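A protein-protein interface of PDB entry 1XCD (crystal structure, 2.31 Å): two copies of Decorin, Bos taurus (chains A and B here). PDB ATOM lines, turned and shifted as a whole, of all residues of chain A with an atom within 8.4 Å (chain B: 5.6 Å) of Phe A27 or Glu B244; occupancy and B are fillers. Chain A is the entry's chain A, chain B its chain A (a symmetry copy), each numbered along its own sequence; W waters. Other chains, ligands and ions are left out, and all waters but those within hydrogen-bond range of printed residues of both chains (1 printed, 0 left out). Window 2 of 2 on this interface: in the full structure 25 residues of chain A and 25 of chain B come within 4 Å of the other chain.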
ATOM      1  N   VAL A  24       4.126  18.805  29.075  1.00  0.00           N
ATOM      2  CA  VAL A  24       5.071  18.436  28.029  1.00  0.00           C
ATOM      3  C   VAL A  24       6.400  17.903  28.552  1.00  0.00           C
ATOM      4  O   VAL A  24       6.888  18.304  29.611  1.00  0.00           O
ATOM      5  CB  VAL A  24       5.378  19.626  27.090  1.00  0.00           C
ATOM      6  CG1 VAL A  24       4.088  20.209  26.540  1.00  0.00           C
ATOM      7  CG2 VAL A  24       6.175  20.680  27.830  1.00  0.00           C
ATOM      8  N   CYS A  25       6.972  16.983  27.786  1.00  0.00           N
ATOM      9  CA  CYS A  25       8.259  16.391  28.097  1.00  0.00           C
ATOM     10  C   CYS A  25       9.237  17.181  27.227  1.00  0.00           C
ATOM     11  O   CYS A  25       9.111  17.183  26.004  1.00  0.00           O
ATOM     12  CB  CYS A  25       8.262  14.916  27.693  1.00  0.00           C
ATOM     13  SG  CYS A  25       9.684  13.981  28.337  1.00  0.00           S
ATOM     14  N   PRO A  26      10.217  17.871  27.841  1.00  0.00           N
ATOM     15  CA  PRO A  26      11.183  18.657  27.055  1.00  0.00           C
ATOM     16  C   PRO A  26      11.868  17.805  25.988  1.00  0.00           C
ATOM     17  O   PRO A  26      12.036  16.599  26.164  1.00  0.00           O
ATOM     18  CB  PRO A  26      12.170  19.164  28.109  1.00  0.00           C
ATOM     19  CG  PRO A  26      11.372  19.125  29.400  1.00  0.00           C
ATOM     20  CD  PRO A  26      10.597  17.837  29.260  1.00  0.00           C
ATOM     21  N   PHE A  27      12.249  18.428  24.877  1.00  0.00           N
ATOM     22  CA  PHE A  27      12.904  17.704  23.789  1.00  0.00           C
ATOM     23  C   PHE A  27      14.187  17.065  24.305  1.00  0.00           C
ATOM     24  O   PHE A  27      15.021  17.744  24.914  1.00  0.00           O
ATOM     25  CB  PHE A  27      13.227  18.653  22.624  1.00  0.00           C
ATOM     26  CG  PHE A  27      13.476  17.952  21.317  1.00  0.00           C
ATOM     27  CD1 PHE A  27      14.759  17.913  20.758  1.00  0.00           C
ATOM     28  CD2 PHE A  27      12.425  17.335  20.634  1.00  0.00           C
ATOM     29  CE1 PHE A  27      14.990  17.266  19.535  1.00  0.00           C
ATOM     30  CE2 PHE A  27      12.639  16.688  19.415  1.00  0.00           C
ATOM     31  CZ  PHE A  27      13.933  16.654  18.863  1.00  0.00           C
ATOM     32  N   ARG A  28      14.315  15.760  24.057  1.00  0.00           N
ATOM     33  CA  ARG A  28      15.453  14.939  24.469  1.00  0.00           C
ATOM     34  C   ARG A  28      15.287  14.318  25.845  1.00  0.00           C
ATOM     35  O   ARG A  28      15.958  13.335  26.147  1.00  0.00           O
ATOM     36  CB  ARG A  28      16.758  15.732  24.431  1.00  0.00           C
ATOM     37  CG  ARG A  28      17.209  16.096  23.040  1.00  0.00           C
ATOM     38  CD  ARG A  28      18.417  17.003  23.113  1.00  0.00           C
ATOM     39  NE  ARG A  28      18.102  18.184  23.907  1.00  0.00           N
ATOM     40  CZ  ARG A  28      18.995  19.086  24.284  1.00  0.00           C
ATOM     41  NH1 ARG A  28      20.271  18.948  23.936  1.00  0.00           N
ATOM     42  NH2 ARG A  28      18.609  20.127  25.014  1.00  0.00           N
ATOM     43  N   CYS A  29      14.414  14.869  26.686  1.00  0.00           N
ATOM     44  CA  CYS A  29      14.236  14.274  28.008  1.00  0.00           C
ATOM     45  C   CYS A  29      13.324  13.070  27.831  1.00  0.00           C
ATOM     46  O   CYS A  29      12.586  12.977  26.853  1.00  0.00           O
ATOM     47  CB  CYS A  29      13.561  15.226  29.015  1.00  0.00           C
ATOM     48  SG  CYS A  29      14.302  16.843  29.471  1.00  0.00           S
ATOM     49  N   GLN A  30      13.373  12.154  28.787  1.00  0.00           N
ATOM     50  CA  GLN A  30      12.538  10.970  28.754  1.00  0.00           C
ATOM     51  C   GLN A  30      11.572  11.084  29.934  1.00  0.00           C
ATOM     52  O   GLN A  30      12.004  11.317  31.061  1.00  0.00           O
ATOM     53  CB  GLN A  30      13.391   9.705  28.894  1.00  0.00           C
ATOM     54  CG  GLN A  30      14.555   9.601  27.906  1.00  0.00           C
ATOM     55  CD  GLN A  30      15.873  10.177  28.441  1.00  0.00           C
ATOM     56  OE1 GLN A  30      16.524   9.584  29.304  1.00  0.00           O
ATOM     57  NE2 GLN A  30      16.263  11.336  27.928  1.00  0.00           N
ATOM     58  N   CYS A  31      10.274  10.935  29.672  1.00  0.00           N
ATOM     59  CA  CYS A  31       9.259  11.027  30.720  1.00  0.00           C
ATOM     60  C   CYS A  31       8.472   9.727  30.776  1.00  0.00           C
ATOM     61  O   CYS A  31       7.545   9.520  29.998  1.00  0.00           O
ATOM     62  CB  CYS A  31       8.336  12.210  30.438  1.00  0.00           C
ATOM     63  SG  CYS A  31       9.255  13.783  30.322  1.00  0.00           S
ATOM     64  N   GLN A  37      13.448  12.388  33.161  1.00  0.00           N
ATOM     65  CA  GLN A  37      14.888  12.256  33.000  1.00  0.00           C
ATOM     66  C   GLN A  37      15.406  13.253  31.993  1.00  0.00           C
ATOM     67  O   GLN A  37      15.153  13.120  30.797  1.00  0.00           O
ATOM     68  CB  GLN A  37      15.210  10.827  32.551  1.00  0.00           C
ATOM     69  CG  GLN A  37      16.682  10.496  32.335  1.00  0.00           C
ATOM     70  CD  GLN A  37      17.572  10.890  33.505  1.00  0.00           C
ATOM     71  OE1 GLN A  37      18.031  12.027  33.584  1.00  0.00           O
ATOM     72  NE2 GLN A  37      17.814   9.953  34.422  1.00  0.00           N
ATOM     73  N   CYS A  38      16.152  14.236  32.487  1.00  0.00           N
ATOM     74  CA  CYS A  38      16.719  15.276  31.648  1.00  0.00           C
ATOM     75  C   CYS A  38      18.222  15.449  31.851  1.00  0.00           C
ATOM     76  O   CYS A  38      18.740  16.547  31.658  1.00  0.00           O
ATOM     77  CB  CYS A  38      16.064  16.612  31.961  1.00  0.00           C
ATOM     78  SG  CYS A  38      14.323  16.867  31.516  1.00  0.00           S
ATOM     79  N   SER A  39      18.923  14.393  32.249  1.00  0.00           N
ATOM     80  CA  SER A  39      20.369  14.495  32.440  1.00  0.00           C
ATOM     81  C   SER A  39      21.083  14.697  31.121  1.00  0.00           C
ATOM     82  O   SER A  39      20.541  14.420  30.058  1.00  0.00           O
ATOM     83  CB  SER A  39      20.947  13.222  33.066  1.00  0.00           C
ATOM     84  OG  SER A  39      20.398  12.951  34.334  1.00  0.00           O
ATOM     85  N   LEU A  41      21.853  17.122  29.117  1.00  0.00           N
ATOM     86  CA  LEU A  41      21.308  17.858  27.982  1.00  0.00           C
ATOM     87  C   LEU A  41      21.776  19.299  27.839  1.00  0.00           C
ATOM     88  O   LEU A  41      21.330  20.002  26.945  1.00  0.00           O
ATOM     89  CB  LEU A  41      19.783  17.848  28.045  1.00  0.00           C
ATOM     90  CG  LEU A  41      19.073  16.499  28.144  1.00  0.00           C
ATOM     91  CD1 LEU A  41      17.561  16.756  28.108  1.00  0.00           C
ATOM     92  CD2 LEU A  41      19.506  15.577  26.999  1.00  0.00           C
ATOM     93  N   LEU A  43      20.912  21.727  29.462  1.00  0.00           N
ATOM     94  CA  LEU A  43      19.832  22.674  29.730  1.00  0.00           C
ATOM     95  C   LEU A  43      20.379  23.860  30.512  1.00  0.00           C
ATOM     96  O   LEU A  43      21.268  23.695  31.350  1.00  0.00           O
ATOM     97  CB  LEU A  43      18.717  22.003  30.528  1.00  0.00           C
ATOM     98  CG  LEU A  43      17.974  20.882  29.814  1.00  0.00           C
ATOM     99  CD1 LEU A  43      16.978  20.284  30.759  1.00  0.00           C
ATOM    100  CD2 LEU A  43      17.276  21.406  28.570  1.00  0.00           C
ATOM    101  N   PRO A  47      13.191  23.068  33.443  1.00  0.00           N
ATOM    102  CA  PRO A  47      12.055  23.019  32.521  1.00  0.00           C
ATOM    103  C   PRO A  47      10.733  23.236  33.257  1.00  0.00           C
ATOM    104  O   PRO A  47      10.587  22.848  34.419  1.00  0.00           O
ATOM    105  CB  PRO A  47      12.153  21.612  31.932  1.00  0.00           C
ATOM    106  CG  PRO A  47      13.628  21.322  31.995  1.00  0.00           C
ATOM    107  CD  PRO A  47      13.982  21.829  33.366  1.00  0.00           C
ATOM    108  N   HIS B 198      17.994  10.991  18.757  1.00  0.00           N
ATOM    109  CA  HIS B 198      18.639  12.265  19.040  1.00  0.00           C
ATOM    110  C   HIS B 198      20.117  12.210  18.716  1.00  0.00           C
ATOM    111  O   HIS B 198      20.861  11.428  19.309  1.00  0.00           O
ATOM    112  CB  HIS B 198      18.435  12.633  20.512  1.00  0.00           C
ATOM    113  CG  HIS B 198      17.002  12.867  20.874  1.00  0.00           C
ATOM    114  ND1 HIS B 198      16.328  14.018  20.531  1.00  0.00           N
ATOM    115  CD2 HIS B 198      16.093  12.067  21.483  1.00  0.00           C
ATOM    116  CE1 HIS B 198      15.067  13.916  20.909  1.00  0.00           C
ATOM    117  NE2 HIS B 198      14.897  12.742  21.490  1.00  0.00           N
ATOM    118  N   ALA B 219       8.999   9.273  15.943  1.00  0.00           N
ATOM    119  CA  ALA B 219       8.174  10.461  16.163  1.00  0.00           C
ATOM    120  C   ALA B 219       9.016  11.730  16.277  1.00  0.00           C
ATOM    121  O   ALA B 219       8.592  12.807  15.868  1.00  0.00           O
ATOM    122  CB  ALA B 219       7.338  10.286  17.442  1.00  0.00           C
ATOM    123  N   LYS B 220      10.205  11.604  16.841  1.00  0.00           N
ATOM    124  CA  LYS B 220      11.066  12.755  17.023  1.00  0.00           C
ATOM    125  C   LYS B 220      12.438  12.479  16.433  1.00  0.00           C
ATOM    126  O   LYS B 220      12.994  11.397  16.610  1.00  0.00           O
ATOM    127  CB  LYS B 220      11.206  13.086  18.510  1.00  0.00           C
ATOM    128  CG  LYS B 220       9.907  13.430  19.242  1.00  0.00           C
ATOM    129  CD  LYS B 220      10.192  13.517  20.742  1.00  0.00           C
ATOM    130  CE  LYS B 220       8.933  13.657  21.594  1.00  0.00           C
ATOM    131  NZ  LYS B 220       8.430  15.052  21.645  1.00  0.00           N
ATOM    132  N   LEU B 221      12.975  13.463  15.727  1.00  0.00           N
ATOM    133  CA  LEU B 221      14.291  13.336  15.108  1.00  0.00           C
ATOM    134  C   LEU B 221      15.071  14.617  15.389  1.00  0.00           C
ATOM    135  O   LEU B 221      14.752  15.675  14.856  1.00  0.00           O
ATOM    136  CB  LEU B 221      14.134  13.119  13.598  1.00  0.00           C
ATOM    137  CG  LEU B 221      15.382  13.106  12.703  1.00  0.00           C
ATOM    138  CD1 LEU B 221      16.362  12.056  13.172  1.00  0.00           C
ATOM    139  CD2 LEU B 221      14.963  12.840  11.251  1.00  0.00           C
ATOM    140  N   GLY B 222      16.073  14.520  16.254  1.00  0.00           N
ATOM    141  CA  GLY B 222      16.876  15.684  16.586  1.00  0.00           C
ATOM    142  C   GLY B 222      18.215  15.669  15.869  1.00  0.00           C
ATOM    143  O   GLY B 222      19.047  14.786  16.117  1.00  0.00           O
ATOM    144  N   LEU B 242       6.839  10.653  11.598  1.00  0.00           N
ATOM    145  CA  LEU B 242       7.640  11.648  12.309  1.00  0.00           C
ATOM    146  C   LEU B 242       6.814  12.903  12.615  1.00  0.00           C
ATOM    147  O   LEU B 242       6.177  13.479  11.740  1.00  0.00           O
ATOM    148  CB  LEU B 242       8.859  12.016  11.463  1.00  0.00           C
ATOM    149  CG  LEU B 242       9.827  13.073  11.994  1.00  0.00           C
ATOM    150  CD1 LEU B 242      10.600  12.514  13.182  1.00  0.00           C
ATOM    151  CD2 LEU B 242      10.784  13.473  10.872  1.00  0.00           C
ATOM    152  N   ARG B 243       6.835  13.334  13.868  1.00  0.00           N
ATOM    153  CA  ARG B 243       6.079  14.510  14.263  1.00  0.00           C
ATOM    154  C   ARG B 243       6.991  15.713  14.522  1.00  0.00           C
ATOM    155  O   ARG B 243       6.590  16.855  14.307  1.00  0.00           O
ATOM    156  CB  ARG B 243       5.249  14.194  15.517  1.00  0.00           C
ATOM    157  CG  ARG B 243       4.416  15.359  16.032  1.00  0.00           C
ATOM    158  CD  ARG B 243       3.464  14.945  17.170  1.00  0.00           C
ATOM    159  NE  ARG B 243       4.161  14.503  18.380  1.00  0.00           N
ATOM    160  CZ  ARG B 243       4.433  13.235  18.693  1.00  0.00           C
ATOM    161  NH1 ARG B 243       4.066  12.241  17.890  1.00  0.00           N
ATOM    162  NH2 ARG B 243       5.083  12.960  19.821  1.00  0.00           N
ATOM    163  N   GLU B 244       8.218  15.465  14.971  1.00  0.00           N
ATOM    164  CA  GLU B 244       9.138  16.565  15.262  1.00  0.00           C
ATOM    165  C   GLU B 244      10.493  16.457  14.590  1.00  0.00           C
ATOM    166  O   GLU B 244      11.218  15.470  14.762  1.00  0.00           O
ATOM    167  CB  GLU B 244       9.373  16.698  16.763  1.00  0.00           C
ATOM    168  CG  GLU B 244       8.131  16.899  17.574  1.00  0.00           C
ATOM    169  CD  GLU B 244       8.443  17.453  18.954  1.00  0.00           C
ATOM    170  OE1 GLU B 244       7.788  17.023  19.927  1.00  0.00           O
ATOM    171  OE2 GLU B 244       9.336  18.329  19.052  1.00  0.00           O
ATOM    172  N   LEU B 245      10.846  17.500  13.852  1.00  0.00           N
ATOM    173  CA  LEU B 245      12.116  17.542  13.156  1.00  0.00           C
ATOM    174  C   LEU B 245      12.884  18.806  13.547  1.00  0.00           C
ATOM    175  O   LEU B 245      12.457  19.913  13.242  1.00  0.00           O
ATOM    176  CB  LEU B 245      11.871  17.515  11.648  1.00  0.00           C
ATOM    177  CG  LEU B 245      13.076  17.565  10.706  1.00  0.00           C
ATOM    178  CD1 LEU B 245      14.020  16.409  10.989  1.00  0.00           C
ATOM    179  CD2 LEU B 245      12.580  17.509   9.266  1.00  0.00           C
ATOM    180  N   HIS B 246      14.001  18.635  14.246  1.00  0.00           N
ATOM    181  CA  HIS B 246      14.830  19.768  14.645  1.00  0.00           C
ATOM    182  C   HIS B 246      16.092  19.717  13.807  1.00  0.00           C
ATOM    183  O   HIS B 246      16.908  18.803  13.959  1.00  0.00           O
ATOM    184  CB  HIS B 246      15.244  19.697  16.120  1.00  0.00           C
ATOM    185  CG  HIS B 246      14.121  19.877  17.087  1.00  0.00           C
ATOM    186  ND1 HIS B 246      14.319  20.347  18.367  1.00  0.00           N
ATOM    187  CD2 HIS B 246      12.797  19.620  16.982  1.00  0.00           C
ATOM    188  CE1 HIS B 246      13.166  20.374  19.008  1.00  0.00           C
ATOM    189  NE2 HIS B 246      12.226  19.935  18.190  1.00  0.00           N
ATOM    190  N   ILE B 265       4.270  15.128   9.991  1.00  0.00           N
ATOM    191  CA  ILE B 265       5.173  16.167  10.491  1.00  0.00           C
ATOM    192  C   ILE B 265       4.405  17.393  11.005  1.00  0.00           C
ATOM    193  O   ILE B 265       3.549  17.935  10.320  1.00  0.00           O
ATOM    194  CB  ILE B 265       6.200  16.595   9.398  1.00  0.00           C
ATOM    195  CG1 ILE B 265       7.232  17.548   9.992  1.00  0.00           C
ATOM    196  CG2 ILE B 265       5.495  17.264   8.236  1.00  0.00           C
ATOM    197  CD1 ILE B 265       8.078  16.927  11.068  1.00  0.00           C
ATOM    198  N   GLN B 266       4.709  17.828  12.221  1.00  0.00           N
ATOM    199  CA  GLN B 266       4.013  18.977  12.799  1.00  0.00           C
ATOM    200  C   GLN B 266       4.934  20.077  13.310  1.00  0.00           C
ATOM    201  O   GLN B 266       4.535  21.240  13.376  1.00  0.00           O
ATOM    202  CB  GLN B 266       3.104  18.515  13.948  1.00  0.00           C
ATOM    203  CG  GLN B 266       1.901  17.703  13.493  1.00  0.00           C
ATOM    204  CD  GLN B 266       0.910  17.433  14.620  1.00  0.00           C
ATOM    205  OE1 GLN B 266       1.008  16.428  15.333  1.00  0.00           O
ATOM    206  NE2 GLN B 266      -0.048  18.344  14.788  1.00  0.00           N
ATOM    207  N   VAL B 267       6.153  19.696  13.685  1.00  0.00           N
ATOM    208  CA  VAL B 267       7.151  20.621  14.209  1.00  0.00           C
ATOM    209  C   VAL B 267       8.420  20.549  13.369  1.00  0.00           C
ATOM    210  O   VAL B 267       9.080  19.519  13.336  1.00  0.00           O
ATOM    211  CB  VAL B 267       7.547  20.267  15.673  1.00  0.00           C
ATOM    212  CG1 VAL B 267       8.637  21.212  16.167  1.00  0.00           C
ATOM    213  CG2 VAL B 267       6.343  20.337  16.577  1.00  0.00           C
HETATM  214  O   HOH W   1      10.084  15.243  23.774  1.00  0.00           O
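Water W1 lies within hydrogen-bond range of the side-chain amino group (NZ) of Lys B220 (2.7 Å), the backbone carbonyl oxygen (O) of Cys A25 (3.1 Å) and the backbone carbonyl oxygen (O) of Pro A26 (3.4 Å).
Printed residues of chain B within 4 Å of Phe A27: His B198, Lys B220, Gly B222, Glu B244 and His B246.
Of chain A, only Phe A27 (3.6 Å) comes within 4 Å of Glu B244.
Of the printed residues of chain A, His B246 touches Phe A27.
Of the printed residues of chain A, Gly B222 touches Phe A27.
Printed residues of chain B within 4 Å of Arg A28: His B198.
Printed residues of chain A within 4 Å of His B198: Phe A27 and Arg A28.
Of the printed residues of chain A, Lys B220 touches Phe A27.
The nearest printed residue of chain B that does not touch Phe A27 is Leu B221 (4.2 Å).
The nearest residue of chain A that does not touch Glu B244 is Cys A25 (6.2 Å).
The nearest printed residue of chain A that does not touch Gly B222 is Arg A28 (6.5 Å).
Of the 13 printed residues of chain B, 5 touch a printed residue of chain A.
Printed residues of chain B that touch a printed residue of chain A: His B198, Lys B220, Gly B222, Glu B244 and His B246.
Hydrophobic or aromatic side chains of chain B within 4 Å of the printed part of chain A: His B198 and His B246.
Of the 14 printed residues of chain A, 2 touch a printed residue of chain B.
Hydrophobic or aromatic side chains of chain A that line the printed part of chain B: Phe A27.
Among the printed residues, 6 pairs touch across the chains.
Among the printed residues, no Asp or Glu carboxylate lies within 4 Å of a Lys or Arg side-chain nitrogen of the other chain.
CE1 of His B198 touches CZ of Phe A27 (3.6 Å).
CB of Lys B220 touches CE2 of Phe A27, 3.98 Å away.
CE1 of Phe A27 touches CA of Gly B222, 3.8 Å away.
Phe A27 touches Glu B244 (CD2 to OE2, 3.6 Å).
CG of Phe A27 touches CE1 of His B246, at 3.4 Å.
His B198 touches Arg A28 (ND1 to CG, 3.4 Å).
The side-chain carboxylate (OE1) of Glu B244 lies within salt-bridge range of the side-chain amino group (NZ) of Lys B220 (2.7 Å).
N of His B246 is in hydrogen-bond range of O of Leu B221 (3.1 Å).
NE2 of Gln A30 sits at hydrogen-bond distance from O of Arg A28 (2.7 Å).
NH2 of Arg A28 sits at hydrogen-bond distance from O of Leu A41.
OE2 of Glu B244 is in hydrogen-bond range of NE2 of His B246, at 3.4 Å.
O of Ala B219 lies within hydrogen-bond range of N of Glu B244 (2.8 Å).
No position is printed for both chains.
Of the 6 pairs that touch across the chains among the printed residues, none has its exchanged pair printed and touching as well.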
